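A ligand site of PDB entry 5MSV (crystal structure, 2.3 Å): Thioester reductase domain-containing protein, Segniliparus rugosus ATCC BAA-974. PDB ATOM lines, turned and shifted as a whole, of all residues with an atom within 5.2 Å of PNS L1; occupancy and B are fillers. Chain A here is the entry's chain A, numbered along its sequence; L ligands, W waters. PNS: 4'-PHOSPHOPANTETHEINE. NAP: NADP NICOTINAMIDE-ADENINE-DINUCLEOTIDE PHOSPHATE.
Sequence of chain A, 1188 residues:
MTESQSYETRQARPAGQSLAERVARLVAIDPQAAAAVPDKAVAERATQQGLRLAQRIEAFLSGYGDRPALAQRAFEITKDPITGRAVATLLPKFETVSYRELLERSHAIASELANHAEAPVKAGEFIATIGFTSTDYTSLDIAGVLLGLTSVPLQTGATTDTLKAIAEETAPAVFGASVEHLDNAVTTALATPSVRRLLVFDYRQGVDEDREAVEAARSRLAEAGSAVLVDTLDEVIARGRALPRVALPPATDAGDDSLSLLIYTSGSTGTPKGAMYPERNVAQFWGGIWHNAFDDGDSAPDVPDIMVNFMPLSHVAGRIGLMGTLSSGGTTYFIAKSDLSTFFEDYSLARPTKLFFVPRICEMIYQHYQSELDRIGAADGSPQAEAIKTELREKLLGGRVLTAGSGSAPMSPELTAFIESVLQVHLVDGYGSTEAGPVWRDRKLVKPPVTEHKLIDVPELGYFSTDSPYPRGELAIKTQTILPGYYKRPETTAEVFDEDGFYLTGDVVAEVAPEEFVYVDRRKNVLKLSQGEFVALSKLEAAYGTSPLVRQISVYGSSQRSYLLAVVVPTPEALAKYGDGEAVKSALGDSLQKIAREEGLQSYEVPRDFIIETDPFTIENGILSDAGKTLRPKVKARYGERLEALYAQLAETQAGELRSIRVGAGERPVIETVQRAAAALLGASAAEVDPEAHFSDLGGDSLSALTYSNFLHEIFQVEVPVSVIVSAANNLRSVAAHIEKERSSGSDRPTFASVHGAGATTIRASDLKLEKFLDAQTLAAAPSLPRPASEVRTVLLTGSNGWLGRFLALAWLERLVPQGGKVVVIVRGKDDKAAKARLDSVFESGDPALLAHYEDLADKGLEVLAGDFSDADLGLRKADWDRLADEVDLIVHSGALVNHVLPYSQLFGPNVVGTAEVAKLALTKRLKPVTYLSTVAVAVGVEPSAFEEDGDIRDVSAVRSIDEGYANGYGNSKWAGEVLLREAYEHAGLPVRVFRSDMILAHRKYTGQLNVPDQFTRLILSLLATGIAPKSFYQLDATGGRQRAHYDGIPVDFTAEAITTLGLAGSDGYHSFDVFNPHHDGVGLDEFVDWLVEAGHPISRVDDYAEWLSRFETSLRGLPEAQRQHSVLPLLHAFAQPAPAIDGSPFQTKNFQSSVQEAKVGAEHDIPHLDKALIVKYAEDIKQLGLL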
ATOM      1  N   ASP A 701     -15.203   3.982  -5.721  1.00  0.00           N
ATOM      2  CA  ASP A 701     -15.797   3.628  -4.431  1.00  0.00           C
ATOM      3  C   ASP A 701     -15.162   2.313  -3.929  1.00  0.00           C
ATOM      4  O   ASP A 701     -14.243   1.791  -4.564  1.00  0.00           O
ATOM      5  CB  ASP A 701     -17.336   3.560  -4.524  1.00  0.00           C
ATOM      6  CG  ASP A 701     -17.848   2.517  -5.535  1.00  0.00           C
ATOM      7  OD1 ASP A 701     -17.398   1.359  -5.530  1.00  0.00           O
ATOM      8  OD2 ASP A 701     -18.756   2.840  -6.326  1.00  0.00           O
ATOM      9  N   SER A 702     -15.638   1.805  -2.798  1.00  0.00           N
ATOM     10  CA  SER A 702     -15.109   0.548  -2.225  1.00  0.00           C
ATOM     11  C   SER A 702     -15.297  -0.719  -3.105  1.00  0.00           C
ATOM     12  O   SER A 702     -14.523  -1.673  -2.953  1.00  0.00           O
ATOM     13  CB  SER A 702     -15.693   0.296  -0.804  1.00  0.00           C
ATOM     14  OG  SER A 702     -17.116   0.226  -0.801  1.00  0.00           O
ATOM     15  N   LEU A 703     -16.289  -0.713  -3.996  1.00  0.00           N
ATOM     16  CA  LEU A 703     -16.556  -1.877  -4.865  1.00  0.00           C
ATOM     17  C   LEU A 703     -15.765  -1.860  -6.171  1.00  0.00           C
ATOM     18  O   LEU A 703     -15.235  -2.895  -6.581  1.00  0.00           O
ATOM     19  CB  LEU A 703     -18.061  -2.006  -5.148  1.00  0.00           C
ATOM     20  CG  LEU A 703     -18.940  -2.154  -3.892  1.00  0.00           C
ATOM     21  CD1 LEU A 703     -20.388  -2.407  -4.313  1.00  0.00           C
ATOM     22  CD2 LEU A 703     -18.454  -3.240  -2.935  1.00  0.00           C
ATOM     23  N   VAL A 898     -16.379  -1.367   7.725  1.00  0.00           N
ATOM     24  CA  VAL A 898     -17.734  -1.919   7.809  1.00  0.00           C
ATOM     25  C   VAL A 898     -18.261  -2.027   6.398  1.00  0.00           C
ATOM     26  O   VAL A 898     -18.666  -1.029   5.802  1.00  0.00           O
ATOM     27  CB  VAL A 898     -18.645  -1.028   8.660  1.00  0.00           C
ATOM     28  CG1 VAL A 898     -20.042  -1.655   8.806  1.00  0.00           C
ATOM     29  CG2 VAL A 898     -18.022  -0.783  10.020  1.00  0.00           C
ATOM     30  N   ASN A 899     -18.241  -3.235   5.858  1.00  0.00           N
ATOM     31  CA  ASN A 899     -18.600  -3.462   4.461  1.00  0.00           C
ATOM     32  C   ASN A 899     -19.204  -4.859   4.297  1.00  0.00           C
ATOM     33  O   ASN A 899     -18.577  -5.851   4.669  1.00  0.00           O
ATOM     34  CB  ASN A 899     -17.355  -3.280   3.582  1.00  0.00           C
ATOM     35  CG  ASN A 899     -17.690  -3.260   2.109  1.00  0.00           C
ATOM     36  OD1 ASN A 899     -18.222  -4.227   1.566  1.00  0.00           O
ATOM     37  ND2 ASN A 899     -17.368  -2.157   1.440  1.00  0.00           N
ATOM     38  N   HIS A 900     -20.399  -4.915   3.739  1.00  0.00           N
ATOM     39  CA  HIS A 900     -21.200  -6.153   3.648  1.00  0.00           C
ATOM     40  C   HIS A 900     -20.912  -7.008   2.405  1.00  0.00           C
ATOM     41  O   HIS A 900     -21.431  -8.105   2.292  1.00  0.00           O
ATOM     42  CB  HIS A 900     -22.692  -5.790   3.688  1.00  0.00           C
ATOM     43  CG  HIS A 900     -23.167  -5.332   5.032  1.00  0.00           C
ATOM     44  ND1 HIS A 900     -24.478  -4.989   5.290  1.00  0.00           N
ATOM     45  CD2 HIS A 900     -22.501  -5.177   6.206  1.00  0.00           C
ATOM     46  CE1 HIS A 900     -24.603  -4.626   6.552  1.00  0.00           C
ATOM     47  NE2 HIS A 900     -23.422  -4.730   7.135  1.00  0.00           N
ATOM     48  N   VAL A 901     -20.080  -6.502   1.496  1.00  0.00           N
ATOM     49  CA  VAL A 901     -19.749  -7.165   0.235  1.00  0.00           C
ATOM     50  C   VAL A 901     -18.308  -7.693   0.194  1.00  0.00           C
ATOM     51  O   VAL A 901     -18.077  -8.781  -0.334  1.00  0.00           O
ATOM     52  CB  VAL A 901     -19.992  -6.200  -0.944  1.00  0.00           C
ATOM     53  CG1 VAL A 901     -19.568  -6.805  -2.276  1.00  0.00           C
ATOM     54  CG2 VAL A 901     -21.464  -5.830  -0.996  1.00  0.00           C
ATOM     55  N   THR A 935     -20.787  -6.999  16.360  1.00  0.00           N
ATOM     56  CA  THR A 935     -21.935  -6.988  15.470  1.00  0.00           C
ATOM     57  C   THR A 935     -22.756  -8.264  15.602  1.00  0.00           C
ATOM     58  O   THR A 935     -22.209  -9.333  15.891  1.00  0.00           O
ATOM     59  CB  THR A 935     -21.483  -6.810  14.002  1.00  0.00           C
ATOM     60  OG1 THR A 935     -22.605  -6.930  13.122  1.00  0.00           O
ATOM     61  CG2 THR A 935     -20.440  -7.854  13.601  1.00  0.00           C
ATOM     62  N   TYR A 970     -17.336  -9.632   6.729  1.00  0.00           N
ATOM     63  CA  TYR A 970     -17.514  -8.676   7.806  1.00  0.00           C
ATOM     64  C   TYR A 970     -17.750  -9.396   9.139  1.00  0.00           C
ATOM     65  O   TYR A 970     -17.057  -9.129  10.116  1.00  0.00           O
ATOM     66  CB  TYR A 970     -18.657  -7.702   7.486  1.00  0.00           C
ATOM     67  CG  TYR A 970     -19.006  -6.769   8.615  1.00  0.00           C
ATOM     68  CD1 TYR A 970     -18.074  -5.830   9.094  1.00  0.00           C
ATOM     69  CD2 TYR A 970     -20.253  -6.836   9.239  1.00  0.00           C
ATOM     70  CE1 TYR A 970     -18.389  -4.992  10.151  1.00  0.00           C
ATOM     71  CE2 TYR A 970     -20.575  -5.988  10.280  1.00  0.00           C
ATOM     72  CZ  TYR A 970     -19.641  -5.068  10.747  1.00  0.00           C
ATOM     73  OH  TYR A 970     -19.983  -4.260  11.798  1.00  0.00           O
ATOM     74  N   ASP A 998     -26.760  -4.162  16.587  1.00  0.00           N
ATOM     75  CA  ASP A 998     -27.713  -4.371  15.488  1.00  0.00           C
ATOM     76  C   ASP A 998     -27.572  -3.149  14.548  1.00  0.00           C
ATOM     77  O   ASP A 998     -26.516  -2.537  14.524  1.00  0.00           O
ATOM     78  CB  ASP A 998     -29.133  -4.524  16.065  1.00  0.00           C
ATOM     79  CG  ASP A 998     -29.618  -3.286  16.862  1.00  0.00           C
ATOM     80  OD1 ASP A 998     -28.808  -2.386  17.200  1.00  0.00           O
ATOM     81  OD2 ASP A 998     -30.826  -3.241  17.184  1.00  0.00           O
ATOM     82  N   MET A 999     -28.615  -2.797  13.799  1.00  0.00           N
ATOM     83  CA  MET A 999     -28.618  -1.568  13.017  1.00  0.00           C
ATOM     84  C   MET A 999     -28.752  -0.342  13.945  1.00  0.00           C
ATOM     85  O   MET A 999     -29.769  -0.183  14.635  1.00  0.00           O
ATOM     86  CB  MET A 999     -29.745  -1.585  11.974  1.00  0.00           C
ATOM     87  CG  MET A 999     -29.558  -0.587  10.842  1.00  0.00           C
ATOM     88  SD  MET A 999     -28.182  -0.935   9.712  1.00  0.00           S
ATOM     89  CE  MET A 999     -28.605  -2.583   9.127  1.00  0.00           C
ATOM     90  N   ASN A1011     -26.853   7.350   9.522  1.00  0.00           N
ATOM     91  CA  ASN A1011     -25.785   6.600   8.882  1.00  0.00           C
ATOM     92  C   ASN A1011     -26.129   6.451   7.413  1.00  0.00           C
ATOM     93  O   ASN A1011     -26.869   5.542   7.026  1.00  0.00           O
ATOM     94  CB  ASN A1011     -25.611   5.230   9.552  1.00  0.00           C
ATOM     95  CG  ASN A1011     -24.308   4.553   9.174  1.00  0.00           C
ATOM     96  OD1 ASN A1011     -23.558   5.052   8.323  1.00  0.00           O
ATOM     97  ND2 ASN A1011     -24.021   3.414   9.791  1.00  0.00           N
ATOM     98  N   PRO A1013     -24.537   5.552   4.528  1.00  0.00           N
ATOM     99  CA  PRO A1013     -24.301   4.326   3.765  1.00  0.00           C
ATOM    100  C   PRO A1013     -24.900   3.008   4.321  1.00  0.00           C
ATOM    101  O   PRO A1013     -24.767   1.981   3.649  1.00  0.00           O
ATOM    102  CB  PRO A1013     -22.770   4.239   3.733  1.00  0.00           C
ATOM    103  CG  PRO A1013     -22.334   4.923   4.977  1.00  0.00           C
ATOM    104  CD  PRO A1013     -23.297   6.059   5.146  1.00  0.00           C
ATOM    105  N   ASP A1014     -25.557   3.014   5.479  1.00  0.00           N
ATOM    106  CA  ASP A1014     -26.083   1.749   6.021  1.00  0.00           C
ATOM    107  C   ASP A1014     -27.274   1.211   5.225  1.00  0.00           C
ATOM    108  O   ASP A1014     -27.910   1.935   4.447  1.00  0.00           O
ATOM    109  CB  ASP A1014     -26.300   1.775   7.564  1.00  0.00           C
ATOM    110  CG  ASP A1014     -27.687   2.283   8.018  1.00  0.00           C
ATOM    111  OD1 ASP A1014     -28.620   2.457   7.213  1.00  0.00           O
ATOM    112  OD2 ASP A1014     -27.843   2.490   9.253  1.00  0.00           O
ATOM    113  N   GLN A1015     -27.539  -0.066   5.426  1.00  0.00           N
ATOM    114  CA  GLN A1015     -28.570  -0.796   4.679  1.00  0.00           C
ATOM    115  C   GLN A1015     -29.978  -0.212   4.887  1.00  0.00           C
ATOM    116  O   GLN A1015     -30.749  -0.102   3.932  1.00  0.00           O
ATOM    117  CB  GLN A1015     -28.553  -2.258   5.103  1.00  0.00           C
ATOM    118  CG  GLN A1015     -29.385  -3.197   4.239  1.00  0.00           C
ATOM    119  CD  GLN A1015     -29.533  -4.558   4.888  1.00  0.00           C
ATOM    120  OE1 GLN A1015     -29.029  -5.559   4.372  1.00  0.00           O
ATOM    121  NE2 GLN A1015     -30.188  -4.606   6.038  1.00  0.00           N
ATOM    122  N   ARG A1018     -30.275   3.328   3.162  1.00  0.00           N
ATOM    123  CA  ARG A1018     -30.366   3.014   1.740  1.00  0.00           C
ATOM    124  C   ARG A1018     -31.759   2.527   1.343  1.00  0.00           C
ATOM    125  O   ARG A1018     -32.307   2.971   0.333  1.00  0.00           O
ATOM    126  CB  ARG A1018     -29.304   1.978   1.347  1.00  0.00           C
ATOM    127  CG  ARG A1018     -27.881   2.523   1.291  1.00  0.00           C
ATOM    128  CD  ARG A1018     -26.870   1.407   1.123  1.00  0.00           C
ATOM    129  NE  ARG A1018     -25.500   1.907   1.089  1.00  0.00           N
ATOM    130  CZ  ARG A1018     -24.909   2.511   0.049  1.00  0.00           C
ATOM    131  NH1 ARG A1018     -25.554   2.704  -1.091  1.00  0.00           N
ATOM    132  NH2 ARG A1018     -23.662   2.924   0.157  1.00  0.00           N
ATOM    133  N   PRO A1130     -26.661  -1.771  -4.519  1.00  0.00           N
ATOM    134  CA  PRO A1130     -25.537  -2.704  -4.291  1.00  0.00           C
ATOM    135  C   PRO A1130     -25.739  -3.764  -3.188  1.00  0.00           C
ATOM    136  O   PRO A1130     -24.931  -4.681  -3.081  1.00  0.00           O
ATOM    137  CB  PRO A1130     -24.379  -1.764  -3.928  1.00  0.00           C
ATOM    138  CG  PRO A1130     -25.030  -0.525  -3.416  1.00  0.00           C
ATOM    139  CD  PRO A1130     -26.286  -0.372  -4.210  1.00  0.00           C
ATOM    140  N   LEU A1131     -26.779  -3.607  -2.365  1.00  0.00           N
ATOM    141  CA  LEU A1131     -27.138  -4.596  -1.348  1.00  0.00           C
ATOM    142  C   LEU A1131     -28.482  -5.277  -1.634  1.00  0.00           C
ATOM    143  O   LEU A1131     -29.031  -5.937  -0.734  1.00  0.00           O
ATOM    144  CB  LEU A1131     -27.195  -3.926   0.028  1.00  0.00           C
ATOM    145  CG  LEU A1131     -25.934  -3.201   0.516  1.00  0.00           C
ATOM    146  CD1 LEU A1131     -26.243  -2.500   1.839  1.00  0.00           C
ATOM    147  CD2 LEU A1131     -24.764  -4.145   0.679  1.00  0.00           C
HETATM  148  O23 PNS L   1     -18.871   1.942  -1.800  1.00  0.00           O
HETATM  149  P24 PNS L   1     -18.351   1.060  -0.699  1.00  0.00           P
HETATM  150  O26 PNS L   1     -17.896   1.703   0.587  1.00  0.00           O
HETATM  151  O27 PNS L   1     -19.397  -0.138  -0.366  1.00  0.00           O
HETATM  152  C28 PNS L   1     -20.804  -0.017  -0.584  1.00  0.00           C
HETATM  153  C29 PNS L   1     -21.566  -0.908   0.403  1.00  0.00           C
HETATM  154  C30 PNS L   1     -23.059  -0.790   0.085  1.00  0.00           C
HETATM  155  C31 PNS L   1     -21.122  -2.353   0.189  1.00  0.00           C
HETATM  156  C32 PNS L   1     -21.271  -0.449   1.854  1.00  0.00           C
HETATM  157  O33 PNS L   1     -21.672   0.923   2.029  1.00  0.00           O
HETATM  158  C34 PNS L   1     -21.961  -1.271   2.910  1.00  0.00           C
HETATM  159  O35 PNS L   1     -21.533  -2.381   3.179  1.00  0.00           O
HETATM  160  N36 PNS L   1     -23.015  -0.686   3.519  1.00  0.00           N
HETATM  161  C37 PNS L   1     -23.778  -1.248   4.626  1.00  0.00           C
HETATM  162  C38 PNS L   1     -23.224  -0.782   5.962  1.00  0.00           C
HETATM  163  C39 PNS L   1     -24.136  -1.068   7.139  1.00  0.00           C
HETATM  164  O40 PNS L   1     -25.293  -1.452   6.956  1.00  0.00           O
HETATM  165  N41 PNS L   1     -23.590  -0.838   8.351  1.00  0.00           N
HETATM  166  C42 PNS L   1     -24.273  -0.946   9.641  1.00  0.00           C
HETATM  167  C43 PNS L   1     -24.710  -2.359  10.029  1.00  0.00           C
HETATM  168  S44 PNS L   1     -23.300  -3.434  10.390  1.00  0.00           S
HETATM  169  PA  NAP L   2     -18.393   3.418  10.149  1.00  0.00           P
HETATM  170  O1A NAP L   2     -19.341   4.567  10.232  1.00  0.00           O
HETATM  171  O2A NAP L   2     -18.131   2.729   8.842  1.00  0.00           O
HETATM  172  O5B NAP L   2     -17.026   3.957  10.753  1.00  0.00           O
HETATM  173  C5B NAP L   2     -15.818   3.224  10.673  1.00  0.00           C
HETATM  174  C4B NAP L   2     -14.731   4.077  11.317  1.00  0.00           C
HETATM  175  O4B NAP L   2     -13.500   3.349  11.418  1.00  0.00           O
HETATM  176  C3B NAP L   2     -14.414   5.284  10.437  1.00  0.00           C
HETATM  177  O3B NAP L   2     -14.037   6.388  11.257  1.00  0.00           O
HETATM  178  C2B NAP L   2     -13.238   4.820   9.631  1.00  0.00           C
HETATM  179  O2B NAP L   2     -12.471   5.870   9.062  1.00  0.00           O
HETATM  180  C1B NAP L   2     -12.483   4.074  10.728  1.00  0.00           C
HETATM  181  N9A NAP L   2     -11.431   3.214  10.157  1.00  0.00           N
HETATM  182  C8A NAP L   2     -11.573   2.216   9.266  1.00  0.00           C
HETATM  183  N7A NAP L   2     -10.357   1.684   8.964  1.00  0.00           N
HETATM  184  C5A NAP L   2      -9.446   2.357   9.657  1.00  0.00           C
HETATM  185  C6A NAP L   2      -7.984   2.294   9.808  1.00  0.00           C
HETATM  186  N6A NAP L   2      -7.280   1.378   9.114  1.00  0.00           N
HETATM  187  N1A NAP L   2      -7.393   3.169  10.644  1.00  0.00           N
HETATM  188  C2A NAP L   2      -8.101   4.107  11.329  1.00  0.00           C
HETATM  189  N3A NAP L   2      -9.439   4.222  11.239  1.00  0.00           N
HETATM  190  C4A NAP L   2     -10.145   3.382  10.439  1.00  0.00           C
HETATM  191  O3  NAP L   2     -18.764   2.266  11.212  1.00  0.00           O
HETATM  192  PN  NAP L   2     -19.938   2.385  12.314  1.00  0.00           P
HETATM  193  O1N NAP L   2     -21.242   2.158  11.616  1.00  0.00           O
HETATM  194  O2N NAP L   2     -19.694   3.645  13.113  1.00  0.00           O
HETATM  195  O5D NAP L   2     -19.653   1.101  13.233  1.00  0.00           O
HETATM  196  C5D NAP L   2     -19.007   1.202  14.497  1.00  0.00           C
HETATM  197  C4D NAP L   2     -18.516  -0.154  14.991  1.00  0.00           C
HETATM  198  O4D NAP L   2     -19.647  -0.995  15.313  1.00  0.00           O
HETATM  199  C3D NAP L   2     -17.684  -0.911  13.969  1.00  0.00           C
HETATM  200  O3D NAP L   2     -16.488  -1.428  14.549  1.00  0.00           O
HETATM  201  C2D NAP L   2     -18.593  -2.027  13.511  1.00  0.00           C
HETATM  202  O2D NAP L   2     -17.890  -3.186  13.073  1.00  0.00           O
HETATM  203  C1D NAP L   2     -19.445  -2.292  14.748  1.00  0.00           C
HETATM  204  N1N NAP L   2     -20.735  -2.880  14.406  1.00  0.00           N
HETATM  205  P2B NAP L   2     -12.496   6.306   7.519  1.00  0.00           P
HETATM  206  O1X NAP L   2     -12.939   5.108   6.710  1.00  0.00           O
HETATM  207  O2X NAP L   2     -13.473   7.475   7.426  1.00  0.00           O
HETATM  208  O3X NAP L   2     -11.052   6.708   7.316  1.00  0.00           O
HETATM  209  O   HOH W   1     -21.781   1.536   9.092  1.00  0.00           O
HETATM  210  O   HOH W   2     -23.916  -4.310  13.208  1.00  0.00           O
HETATM  211  O   HOH W   3     -16.512   0.323   2.445  1.00  0.00           O
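Residues that only touch PNS L1: Asp 1014 (3.4 Å), Asp 701 (3.5 Å), Val 898 (3.7 Å), Val 901 (3.7 Å), Met 999 (3.8 Å) and Leu 1131 (3.8 Å).
The backbone NH (N) of Ser 702 is in hydrogen-bond range of an oxygen (O23) of PNS L1, 3.4 Å away. An oxygen (O2D) of NAP L2 lies within hydrogen-bond range of the side-chain hydroxyl (OH) of Tyr 970 (2.7 Å). A nitrogen (N36) of PNS L1 sits at hydrogen-bond distance from the backbone carbonyl oxygen (O) of Pro 1013, 3.2 Å away. A sulfur (S44) of PNS L1 lies close to a ring nitrogen (NE2) of His 900 (3.5 Å). An oxygen (O27) of PNS L1 lies within hydrogen-bond range of the side-chain amide nitrogen of Asn 899 (3.4 Å). S44 of PNS L1 lies close to OH of Tyr 970, 3.7 Å away. The side-chain hydroxyl of Ser 702 is bonded to a phosphorus (P24) of PNS L1. The backbone NH of His 900 is in hydrogen-bond range of an oxygen (O35) of PNS L1, at 2.8 Å. O33 of PNS L1 is in hydrogen-bond range of NH2 of Arg 1018 (3.4 Å). An oxygen (O40) of PNS L1 is in hydrogen-bond range of the backbone NH of Gln 1015 (3.1 Å).
The side-chain amide oxygen (OD1) of Asn 899 is in hydrogen-bond range of the backbone NH (N) of Val 901, at 2.9 Å. The backbone carbonyl oxygen of Pro 1013 is in hydrogen-bond range of the guanidinium group of Arg 1018 (2.7 Å). The side-chain amide nitrogen (ND2) of Asn 899 is in hydrogen-bond range of the side-chain hydroxyl (OG) of Ser 702, at 3.3 Å. N of Leu 703 is in hydrogen-bond range of OD1 of Asp 701, at 2.8 Å.
Water W3 lies within hydrogen-bond range of O26 of PNS L1, ND2 of Asn 899 and OG of Ser 702. Water W2 lies within hydrogen-bond range of OG1 of Thr 935 (2.9 Å), S44 of PNS L1 (3.0 Å) and O of Asp 998 (3.4 Å). Water W1 lies within hydrogen-bond range of O1N of NAP L2 (2.7 Å), ND2 of Asn 1011 (3.0 Å) and N41 of PNS L1 (3.1 Å).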
